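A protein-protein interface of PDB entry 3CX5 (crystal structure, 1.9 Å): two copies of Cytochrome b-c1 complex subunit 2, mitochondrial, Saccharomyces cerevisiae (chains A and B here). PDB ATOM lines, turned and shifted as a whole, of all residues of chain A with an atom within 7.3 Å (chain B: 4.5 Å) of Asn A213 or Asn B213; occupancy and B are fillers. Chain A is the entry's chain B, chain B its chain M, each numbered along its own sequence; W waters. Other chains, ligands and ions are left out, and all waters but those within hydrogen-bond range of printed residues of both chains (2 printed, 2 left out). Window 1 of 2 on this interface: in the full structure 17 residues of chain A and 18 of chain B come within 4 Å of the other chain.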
ATOM      1  N   GLN A 129       5.137  31.666  25.990  1.00  0.00           N
ATOM      2  CA  GLN A 129       5.478  30.256  26.159  1.00  0.00           C
ATOM      3  C   GLN A 129       6.776  30.087  26.948  1.00  0.00           C
ATOM      4  O   GLN A 129       6.878  29.218  27.814  1.00  0.00           O
ATOM      5  CB  GLN A 129       5.616  29.590  24.789  1.00  0.00           C
ATOM      6  CG  GLN A 129       4.305  29.406  24.068  1.00  0.00           C
ATOM      7  CD  GLN A 129       3.423  28.406  24.768  1.00  0.00           C
ATOM      8  OE1 GLN A 129       3.793  27.240  24.910  1.00  0.00           O
ATOM      9  NE2 GLN A 129       2.262  28.854  25.238  1.00  0.00           N
ATOM     10  N   LEU A 130       7.759  30.925  26.637  1.00  0.00           N
ATOM     11  CA  LEU A 130       9.047  30.890  27.306  1.00  0.00           C
ATOM     12  C   LEU A 130       8.850  31.182  28.794  1.00  0.00           C
ATOM     13  O   LEU A 130       9.337  30.440  29.646  1.00  0.00           O
ATOM     14  CB  LEU A 130       9.996  31.904  26.659  1.00  0.00           C
ATOM     15  CG  LEU A 130      11.323  31.392  26.079  1.00  0.00           C
ATOM     16  CD1 LEU A 130      11.211  29.957  25.578  1.00  0.00           C
ATOM     17  CD2 LEU A 130      11.787  32.321  24.966  1.00  0.00           C
ATOM     18  N   ALA A 132       6.158  30.825  30.487  1.00  0.00           N
ATOM     19  CA  ALA A 132       5.349  29.743  31.041  1.00  0.00           C
ATOM     20  C   ALA A 132       6.143  28.508  31.449  1.00  0.00           C
ATOM     21  O   ALA A 132       5.978  28.009  32.563  1.00  0.00           O
ATOM     22  CB  ALA A 132       4.250  29.351  30.061  1.00  0.00           C
ATOM     23  N   ILE A 133       6.976  27.990  30.547  1.00  0.00           N
ATOM     24  CA  ILE A 133       7.755  26.793  30.851  1.00  0.00           C
ATOM     25  C   ILE A 133       8.912  27.010  31.825  1.00  0.00           C
ATOM     26  O   ILE A 133       9.316  26.079  32.523  1.00  0.00           O
ATOM     27  CB  ILE A 133       8.282  26.097  29.577  1.00  0.00           C
ATOM     28  CG1 ILE A 133       9.158  27.050  28.762  1.00  0.00           C
ATOM     29  CG2 ILE A 133       7.122  25.544  28.764  1.00  0.00           C
ATOM     30  CD1 ILE A 133       9.731  26.420  27.514  1.00  0.00           C
ATOM     31  N   GLU A 211      13.243  22.555  29.631  1.00  0.00           N
ATOM     32  CA  GLU A 211      11.831  22.418  29.276  1.00  0.00           C
ATOM     33  C   GLU A 211      11.557  22.925  27.858  1.00  0.00           C
ATOM     34  O   GLU A 211      12.250  23.812  27.356  1.00  0.00           O
ATOM     35  CB  GLU A 211      10.956  23.201  30.263  1.00  0.00           C
ATOM     36  CG  GLU A 211      10.970  22.685  31.695  1.00  0.00           C
ATOM     37  CD  GLU A 211      10.189  21.395  31.860  1.00  0.00           C
ATOM     38  OE1 GLU A 211       8.955  21.464  32.045  1.00  0.00           O
ATOM     39  OE2 GLU A 211      10.807  20.310  31.805  1.00  0.00           O
ATOM     40  N   GLU A 212      10.542  22.356  27.215  1.00  0.00           N
ATOM     41  CA  GLU A 212      10.175  22.791  25.874  1.00  0.00           C
ATOM     42  C   GLU A 212       8.686  22.625  25.592  1.00  0.00           C
ATOM     43  O   GLU A 212       8.010  21.801  26.214  1.00  0.00           O
ATOM     44  CB  GLU A 212      11.004  22.064  24.803  1.00  0.00           C
ATOM     45  CG  GLU A 212      10.404  20.768  24.283  1.00  0.00           C
ATOM     46  CD  GLU A 212      11.108  20.249  23.040  1.00  0.00           C
ATOM     47  OE1 GLU A 212      11.601  19.106  23.085  1.00  0.00           O
ATOM     48  OE2 GLU A 212      11.168  20.970  22.018  1.00  0.00           O
ATOM     49  N   ASN A 213       8.182  23.439  24.666  1.00  0.00           N
ATOM     50  CA  ASN A 213       6.781  23.391  24.254  1.00  0.00           C
ATOM     51  C   ASN A 213       6.719  23.722  22.767  1.00  0.00           C
ATOM     52  O   ASN A 213       7.464  24.576  22.273  1.00  0.00           O
ATOM     53  CB  ASN A 213       5.925  24.368  25.068  1.00  0.00           C
ATOM     54  CG  ASN A 213       4.471  23.912  25.187  1.00  0.00           C
ATOM     55  OD1 ASN A 213       4.184  22.842  25.733  1.00  0.00           O
ATOM     56  ND2 ASN A 213       3.552  24.715  24.664  1.00  0.00           N
ATOM     57  N   ARG A 214       5.864  23.002  22.049  1.00  0.00           N
ATOM     58  CA  ARG A 214       5.707  23.192  20.612  1.00  0.00           C
ATOM     59  C   ARG A 214       4.279  23.636  20.283  1.00  0.00           C
ATOM     60  O   ARG A 214       3.313  23.008  20.722  1.00  0.00           O
ATOM     61  CB  ARG A 214       6.071  21.891  19.881  1.00  0.00           C
ATOM     62  CG  ARG A 214       7.467  21.351  20.264  1.00  0.00           C
ATOM     63  CD  ARG A 214       7.840  20.079  19.512  1.00  0.00           C
ATOM     64  NE  ARG A 214       8.248  20.329  18.129  1.00  0.00           N
ATOM     65  CZ  ARG A 214       9.401  20.895  17.770  1.00  0.00           C
ATOM     66  NH1 ARG A 214       9.674  21.075  16.488  1.00  0.00           N
ATOM     67  NH2 ARG A 214      10.280  21.281  18.684  1.00  0.00           N
ATOM     68  N   VAL A 215       4.152  24.707  19.501  1.00  0.00           N
ATOM     69  CA  VAL A 215       2.838  25.249  19.135  1.00  0.00           C
ATOM     70  C   VAL A 215       2.636  25.405  17.627  1.00  0.00           C
ATOM     71  O   VAL A 215       3.356  26.167  16.979  1.00  0.00           O
ATOM     72  CB  VAL A 215       2.614  26.641  19.788  1.00  0.00           C
ATOM     73  CG1 VAL A 215       1.227  27.188  19.437  1.00  0.00           C
ATOM     74  CG2 VAL A 215       2.776  26.555  21.298  1.00  0.00           C
ATOM     75  N   ARG A 216       1.646  24.700  17.080  1.00  0.00           N
ATOM     76  CA  ARG A 216       1.338  24.787  15.651  1.00  0.00           C
ATOM     77  C   ARG A 216       0.756  26.176  15.371  1.00  0.00           C
ATOM     78  O   ARG A 216      -0.075  26.667  16.137  1.00  0.00           O
ATOM     79  CB  ARG A 216       0.334  23.712  15.239  1.00  0.00           C
ATOM     80  CG  ARG A 216       0.712  22.306  15.669  1.00  0.00           C
ATOM     81  CD  ARG A 216       0.055  21.275  14.781  1.00  0.00           C
ATOM     82  NE  ARG A 216       0.658  21.280  13.452  1.00  0.00           N
ATOM     83  CZ  ARG A 216       0.163  20.642  12.400  1.00  0.00           C
ATOM     84  NH1 ARG A 216       0.781  20.703  11.230  1.00  0.00           N
ATOM     85  NH2 ARG A 216      -0.962  19.953  12.513  1.00  0.00           N
ATOM     86  N   ASN A 336      15.684  26.817  28.148  1.00  0.00           N
ATOM     87  CA  ASN A 336      14.372  26.356  27.718  1.00  0.00           C
ATOM     88  C   ASN A 336      14.152  26.737  26.258  1.00  0.00           C
ATOM     89  O   ASN A 336      14.663  27.754  25.791  1.00  0.00           O
ATOM     90  CB  ASN A 336      13.290  26.912  28.645  1.00  0.00           C
ATOM     91  CG  ASN A 336      13.440  26.395  30.073  1.00  0.00           C
ATOM     92  OD1 ASN A 336      13.557  25.187  30.301  1.00  0.00           O
ATOM     93  ND2 ASN A 336      13.477  27.307  31.031  1.00  0.00           N
ATOM     94  N   TYR A 337      13.380  25.920  25.549  1.00  0.00           N
ATOM     95  CA  TYR A 337      13.138  26.123  24.128  1.00  0.00           C
ATOM     96  C   TYR A 337      11.670  25.990  23.690  1.00  0.00           C
ATOM     97  O   TYR A 337      10.938  25.117  24.161  1.00  0.00           O
ATOM     98  CB  TYR A 337      14.020  25.126  23.368  1.00  0.00           C
ATOM     99  CG  TYR A 337      13.809  25.036  21.878  1.00  0.00           C
ATOM    100  CD1 TYR A 337      14.283  26.029  21.021  1.00  0.00           C
ATOM    101  CD2 TYR A 337      13.165  23.934  21.319  1.00  0.00           C
ATOM    102  CE1 TYR A 337      14.124  25.923  19.643  1.00  0.00           C
ATOM    103  CE2 TYR A 337      13.001  23.819  19.948  1.00  0.00           C
ATOM    104  CZ  TYR A 337      13.482  24.814  19.116  1.00  0.00           C
ATOM    105  OH  TYR A 337      13.323  24.692  17.758  1.00  0.00           O
ATOM    106  N   VAL A 338      11.255  26.866  22.780  1.00  0.00           N
ATOM    107  CA  VAL A 338       9.895  26.847  22.242  1.00  0.00           C
ATOM    108  C   VAL A 338       9.911  26.954  20.719  1.00  0.00           C
ATOM    109  O   VAL A 338      10.706  27.708  20.145  1.00  0.00           O
ATOM    110  CB  VAL A 338       9.023  28.002  22.794  1.00  0.00           C
ATOM    111  CG1 VAL A 338       8.722  27.800  24.271  1.00  0.00           C
ATOM    112  CG2 VAL A 338       9.715  29.333  22.569  1.00  0.00           C
ATOM    113  N   ALA A 339       9.067  26.157  20.072  1.00  0.00           N
ATOM    114  CA  ALA A 339       8.941  26.176  18.618  1.00  0.00           C
ATOM    115  C   ALA A 339       7.500  26.562  18.282  1.00  0.00           C
ATOM    116  O   ALA A 339       6.556  25.950  18.781  1.00  0.00           O
ATOM    117  CB  ALA A 339       9.274  24.817  18.032  1.00  0.00           C
ATOM    118  N   VAL A 340       7.334  27.601  17.473  1.00  0.00           N
ATOM    119  CA  VAL A 340       6.003  28.062  17.087  1.00  0.00           C
ATOM    120  C   VAL A 340       5.936  28.169  15.575  1.00  0.00           C
ATOM    121  O   VAL A 340       6.822  28.754  14.953  1.00  0.00           O
ATOM    122  CB  VAL A 340       5.673  29.452  17.714  1.00  0.00           C
ATOM    123  CG1 VAL A 340       4.312  29.959  17.223  1.00  0.00           C
ATOM    124  CG2 VAL A 340       5.681  29.372  19.235  1.00  0.00           C
ATOM    125  N   VAL A 343       6.002  23.565  13.180  1.00  0.00           N
ATOM    126  CA  VAL A 343       6.595  22.672  14.176  1.00  0.00           C
ATOM    127  C   VAL A 343       7.094  21.306  13.699  1.00  0.00           C
ATOM    128  O   VAL A 343       8.058  20.768  14.252  1.00  0.00           O
ATOM    129  CB  VAL A 343       5.622  22.510  15.366  1.00  0.00           C
ATOM    130  CG1 VAL A 343       6.025  21.347  16.248  1.00  0.00           C
ATOM    131  CG2 VAL A 343       5.603  23.800  16.179  1.00  0.00           C
ATOM    132  N   LEU A 349      14.468  20.260  21.139  1.00  0.00           N
ATOM    133  CA  LEU A 349      15.498  20.550  22.138  1.00  0.00           C
ATOM    134  C   LEU A 349      16.614  19.500  22.110  1.00  0.00           C
ATOM    135  O   LEU A 349      17.775  19.818  22.357  1.00  0.00           O
ATOM    136  CB  LEU A 349      14.880  20.650  23.539  1.00  0.00           C
ATOM    137  CG  LEU A 349      15.795  21.035  24.712  1.00  0.00           C
ATOM    138  CD1 LEU A 349      16.601  22.290  24.402  1.00  0.00           C
ATOM    139  CD2 LEU A 349      14.953  21.243  25.960  1.00  0.00           C
ATOM    140  N   GLN B 129      -1.445  15.196  19.836  1.00  0.00           N
ATOM    141  CA  GLN B 129      -0.305  15.641  20.635  1.00  0.00           C
ATOM    142  C   GLN B 129       0.493  14.452  21.175  1.00  0.00           C
ATOM    143  O   GLN B 129       1.722  14.447  21.142  1.00  0.00           O
ATOM    144  CB  GLN B 129      -0.787  16.497  21.807  1.00  0.00           C
ATOM    145  CG  GLN B 129      -1.250  17.884  21.420  1.00  0.00           C
ATOM    146  CD  GLN B 129      -0.117  18.737  20.901  1.00  0.00           C
ATOM    147  OE1 GLN B 129       0.856  18.989  21.614  1.00  0.00           O
ATOM    148  NE2 GLN B 129      -0.225  19.178  19.651  1.00  0.00           N
ATOM    149  N   ILE B 133       4.524  13.850  20.345  1.00  0.00           N
ATOM    150  CA  ILE B 133       5.614  13.809  21.313  1.00  0.00           C
ATOM    151  C   ILE B 133       6.211  12.418  21.535  1.00  0.00           C
ATOM    152  O   ILE B 133       7.390  12.293  21.868  1.00  0.00           O
ATOM    153  CB  ILE B 133       5.224  14.434  22.675  1.00  0.00           C
ATOM    154  CG1 ILE B 133       4.136  13.607  23.362  1.00  0.00           C
ATOM    155  CG2 ILE B 133       4.786  15.882  22.488  1.00  0.00           C
ATOM    156  CD1 ILE B 133       3.759  14.140  24.727  1.00  0.00           C
ATOM    157  N   GLU B 212       6.368  16.002  27.354  1.00  0.00           N
ATOM    158  CA  GLU B 212       5.169  16.740  27.710  1.00  0.00           C
ATOM    159  C   GLU B 212       4.946  17.946  26.796  1.00  0.00           C
ATOM    160  O   GLU B 212       5.900  18.571  26.330  1.00  0.00           O
ATOM    161  CB  GLU B 212       5.280  17.223  29.164  1.00  0.00           C
ATOM    162  CG  GLU B 212       4.193  18.210  29.599  1.00  0.00           C
ATOM    163  CD  GLU B 212       4.390  18.747  31.016  1.00  0.00           C
ATOM    164  OE1 GLU B 212       5.549  19.009  31.417  1.00  0.00           O
ATOM    165  OE2 GLU B 212       3.374  18.923  31.724  1.00  0.00           O
ATOM    166  N   ASN B 213       3.678  18.249  26.528  1.00  0.00           N
ATOM    167  CA  ASN B 213       3.308  19.411  25.723  1.00  0.00           C
ATOM    168  C   ASN B 213       1.961  19.928  26.226  1.00  0.00           C
ATOM    169  O   ASN B 213       1.061  19.148  26.544  1.00  0.00           O
ATOM    170  CB  ASN B 213       3.254  19.086  24.230  1.00  0.00           C
ATOM    171  CG  ASN B 213       3.526  20.310  23.370  1.00  0.00           C
ATOM    172  OD1 ASN B 213       4.608  20.896  23.433  1.00  0.00           O
ATOM    173  ND2 ASN B 213       2.536  20.720  22.586  1.00  0.00           N
ATOM    174  N   ARG B 214       1.852  21.246  26.347  1.00  0.00           N
ATOM    175  CA  ARG B 214       0.637  21.876  26.858  1.00  0.00           C
ATOM    176  C   ARG B 214      -0.013  22.781  25.808  1.00  0.00           C
ATOM    177  O   ARG B 214       0.668  23.565  25.139  1.00  0.00           O
ATOM    178  CB  ARG B 214       0.976  22.658  28.134  1.00  0.00           C
ATOM    179  CG  ARG B 214       1.823  21.842  29.133  1.00  0.00           C
ATOM    180  CD  ARG B 214       2.217  22.639  30.371  1.00  0.00           C
ATOM    181  NE  ARG B 214       1.094  22.847  31.280  1.00  0.00           N
ATOM    182  CZ  ARG B 214       0.543  21.893  32.027  1.00  0.00           C
ATOM    183  NH1 ARG B 214      -0.478  22.182  32.821  1.00  0.00           N
ATOM    184  NH2 ARG B 214       1.016  20.654  31.990  1.00  0.00           N
ATOM    185  N   VAL B 215      -1.333  22.665  25.670  1.00  0.00           N
ATOM    186  CA  VAL B 215      -2.084  23.452  24.685  1.00  0.00           C
ATOM    187  C   VAL B 215      -3.269  24.199  25.299  1.00  0.00           C
ATOM    188  O   VAL B 215      -4.179  23.584  25.862  1.00  0.00           O
ATOM    189  CB  VAL B 215      -2.631  22.547  23.550  1.00  0.00           C
ATOM    190  CG1 VAL B 215      -3.349  23.389  22.486  1.00  0.00           C
ATOM    191  CG2 VAL B 215      -1.506  21.746  22.911  1.00  0.00           C
ATOM    192  N   TYR B 337       2.936  12.876  28.536  1.00  0.00           N
ATOM    193  CA  TYR B 337       1.766  13.592  29.018  1.00  0.00           C
ATOM    194  C   TYR B 337       1.445  14.891  28.281  1.00  0.00           C
ATOM    195  O   TYR B 337       2.341  15.662  27.926  1.00  0.00           O
ATOM    196  CB  TYR B 337       1.979  13.862  30.507  1.00  0.00           C
ATOM    197  CG  TYR B 337       0.951  14.725  31.186  1.00  0.00           C
ATOM    198  CD1 TYR B 337      -0.255  14.190  31.628  1.00  0.00           C
ATOM    199  CD2 TYR B 337       1.213  16.065  31.447  1.00  0.00           C
ATOM    200  CE1 TYR B 337      -1.175  14.971  32.321  1.00  0.00           C
ATOM    201  CE2 TYR B 337       0.305  16.851  32.135  1.00  0.00           C
ATOM    202  CZ  TYR B 337      -0.885  16.301  32.572  1.00  0.00           C
ATOM    203  OH  TYR B 337      -1.770  17.076  33.279  1.00  0.00           O
ATOM    204  N   VAL B 338       0.153  15.129  28.072  1.00  0.00           N
ATOM    205  CA  VAL B 338      -0.308  16.344  27.416  1.00  0.00           C
ATOM    206  C   VAL B 338      -1.494  16.939  28.165  1.00  0.00           C
ATOM    207  O   VAL B 338      -2.385  16.219  28.621  1.00  0.00           O
ATOM    208  CB  VAL B 338      -0.724  16.104  25.943  1.00  0.00           C
ATOM    209  CG1 VAL B 338       0.469  15.646  25.118  1.00  0.00           C
ATOM    210  CG2 VAL B 338      -1.855  15.096  25.867  1.00  0.00           C
ATOM    211  N   ALA B 339      -1.463  18.252  28.342  1.00  0.00           N
ATOM    212  CA  ALA B 339      -2.539  18.967  29.008  1.00  0.00           C
ATOM    213  C   ALA B 339      -3.174  19.878  27.956  1.00  0.00           C
ATOM    214  O   ALA B 339      -2.464  20.541  27.195  1.00  0.00           O
ATOM    215  CB  ALA B 339      -1.990  19.792  30.168  1.00  0.00           C
HETATM  216  O   HOH W   1       2.416  20.829  18.724  1.00  0.00           O
HETATM  217  O   HOH W   2       8.386  19.096  26.841  1.00  0.00           O
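N of Arg A214 is in hydrogen-bond range of OD1 of Asn B213 (2.8 Å).
The side-chain amide oxygen of Asn A213 is in hydrogen-bond range of the backbone NH of Arg B214 (2.9 Å).
The side-chain amide oxygen (OD1) of Asn A213 sits close to the side-chain amide oxygen (OD1) of Asn B213 (3.0 Å).
The backbone carbonyl oxygen of Tyr B337 sits at hydrogen-bond distance from the backbone NH of Asn B213 (3.2 Å).
The side-chain amide nitrogen of Asn B213 is in hydrogen-bond range of the side-chain amide oxygen of Gln B129.
The guanidinium group (NH2) of Arg B214 is in salt-bridge range of the side-chain carboxylate (OE2) of Glu B212, 2.9 Å away.
The backbone carbonyl oxygen (O) of Asn A213 is in hydrogen-bond range of the backbone NH (N) of Ala A339 (3.1 Å).
O of Asn B213 lies within hydrogen-bond range of N of Ala B339 (3.2 Å).
The guanidinium group (NH1) of Arg A214 sits at hydrogen-bond distance from the backbone carbonyl oxygen (O) of Val A343.
Among the printed residues, merely in contact across the chains: Glu A212 with Glu B212 (3.9 Å).
Printed residues of chain B within 4 Å of Glu A212: Glu B212.
Asn A213 touches two residues of chain B.
Of the printed residues of chain B, Arg A214 touches Asn B213.
Of the printed residues of chain A, Glu B212 touches Glu A212.
Asn B213 touches two residues of chain A.
Printed residues of chain A within 4 Å of Arg B214: Asn A213.
Ala B339 touches none of the printed residues of chain A.
The nearest printed residue of chain A that does not touch Glu B212 is Glu A211 (4.2 Å).
Printed residues of chain A that touch a printed residue of chain B: Glu A212, Asn A213 and Arg A214.
Of the 9 printed residues of chain B, 3 touch a printed residue of chain A.
Among the printed residues, no Asp or Glu carboxylate lies within 4 Å of a Lys or Arg side-chain nitrogen of the other chain.
Glu B212 touches its own counterpart, Glu A212.
Asn B213 touches its own counterpart, Asn A213.
Asn A213 touches Arg B214, and with the chains exchanged Arg A214 touches Asn B213.
Water W2 bridges the backbone carbonyl oxygen of Glu B212 and the backbone carbonyl oxygen of Glu A212.
Water W1 bridges O of Arg A214 (3.1 Å) and NE2 of Gln B129 (3.2 Å).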
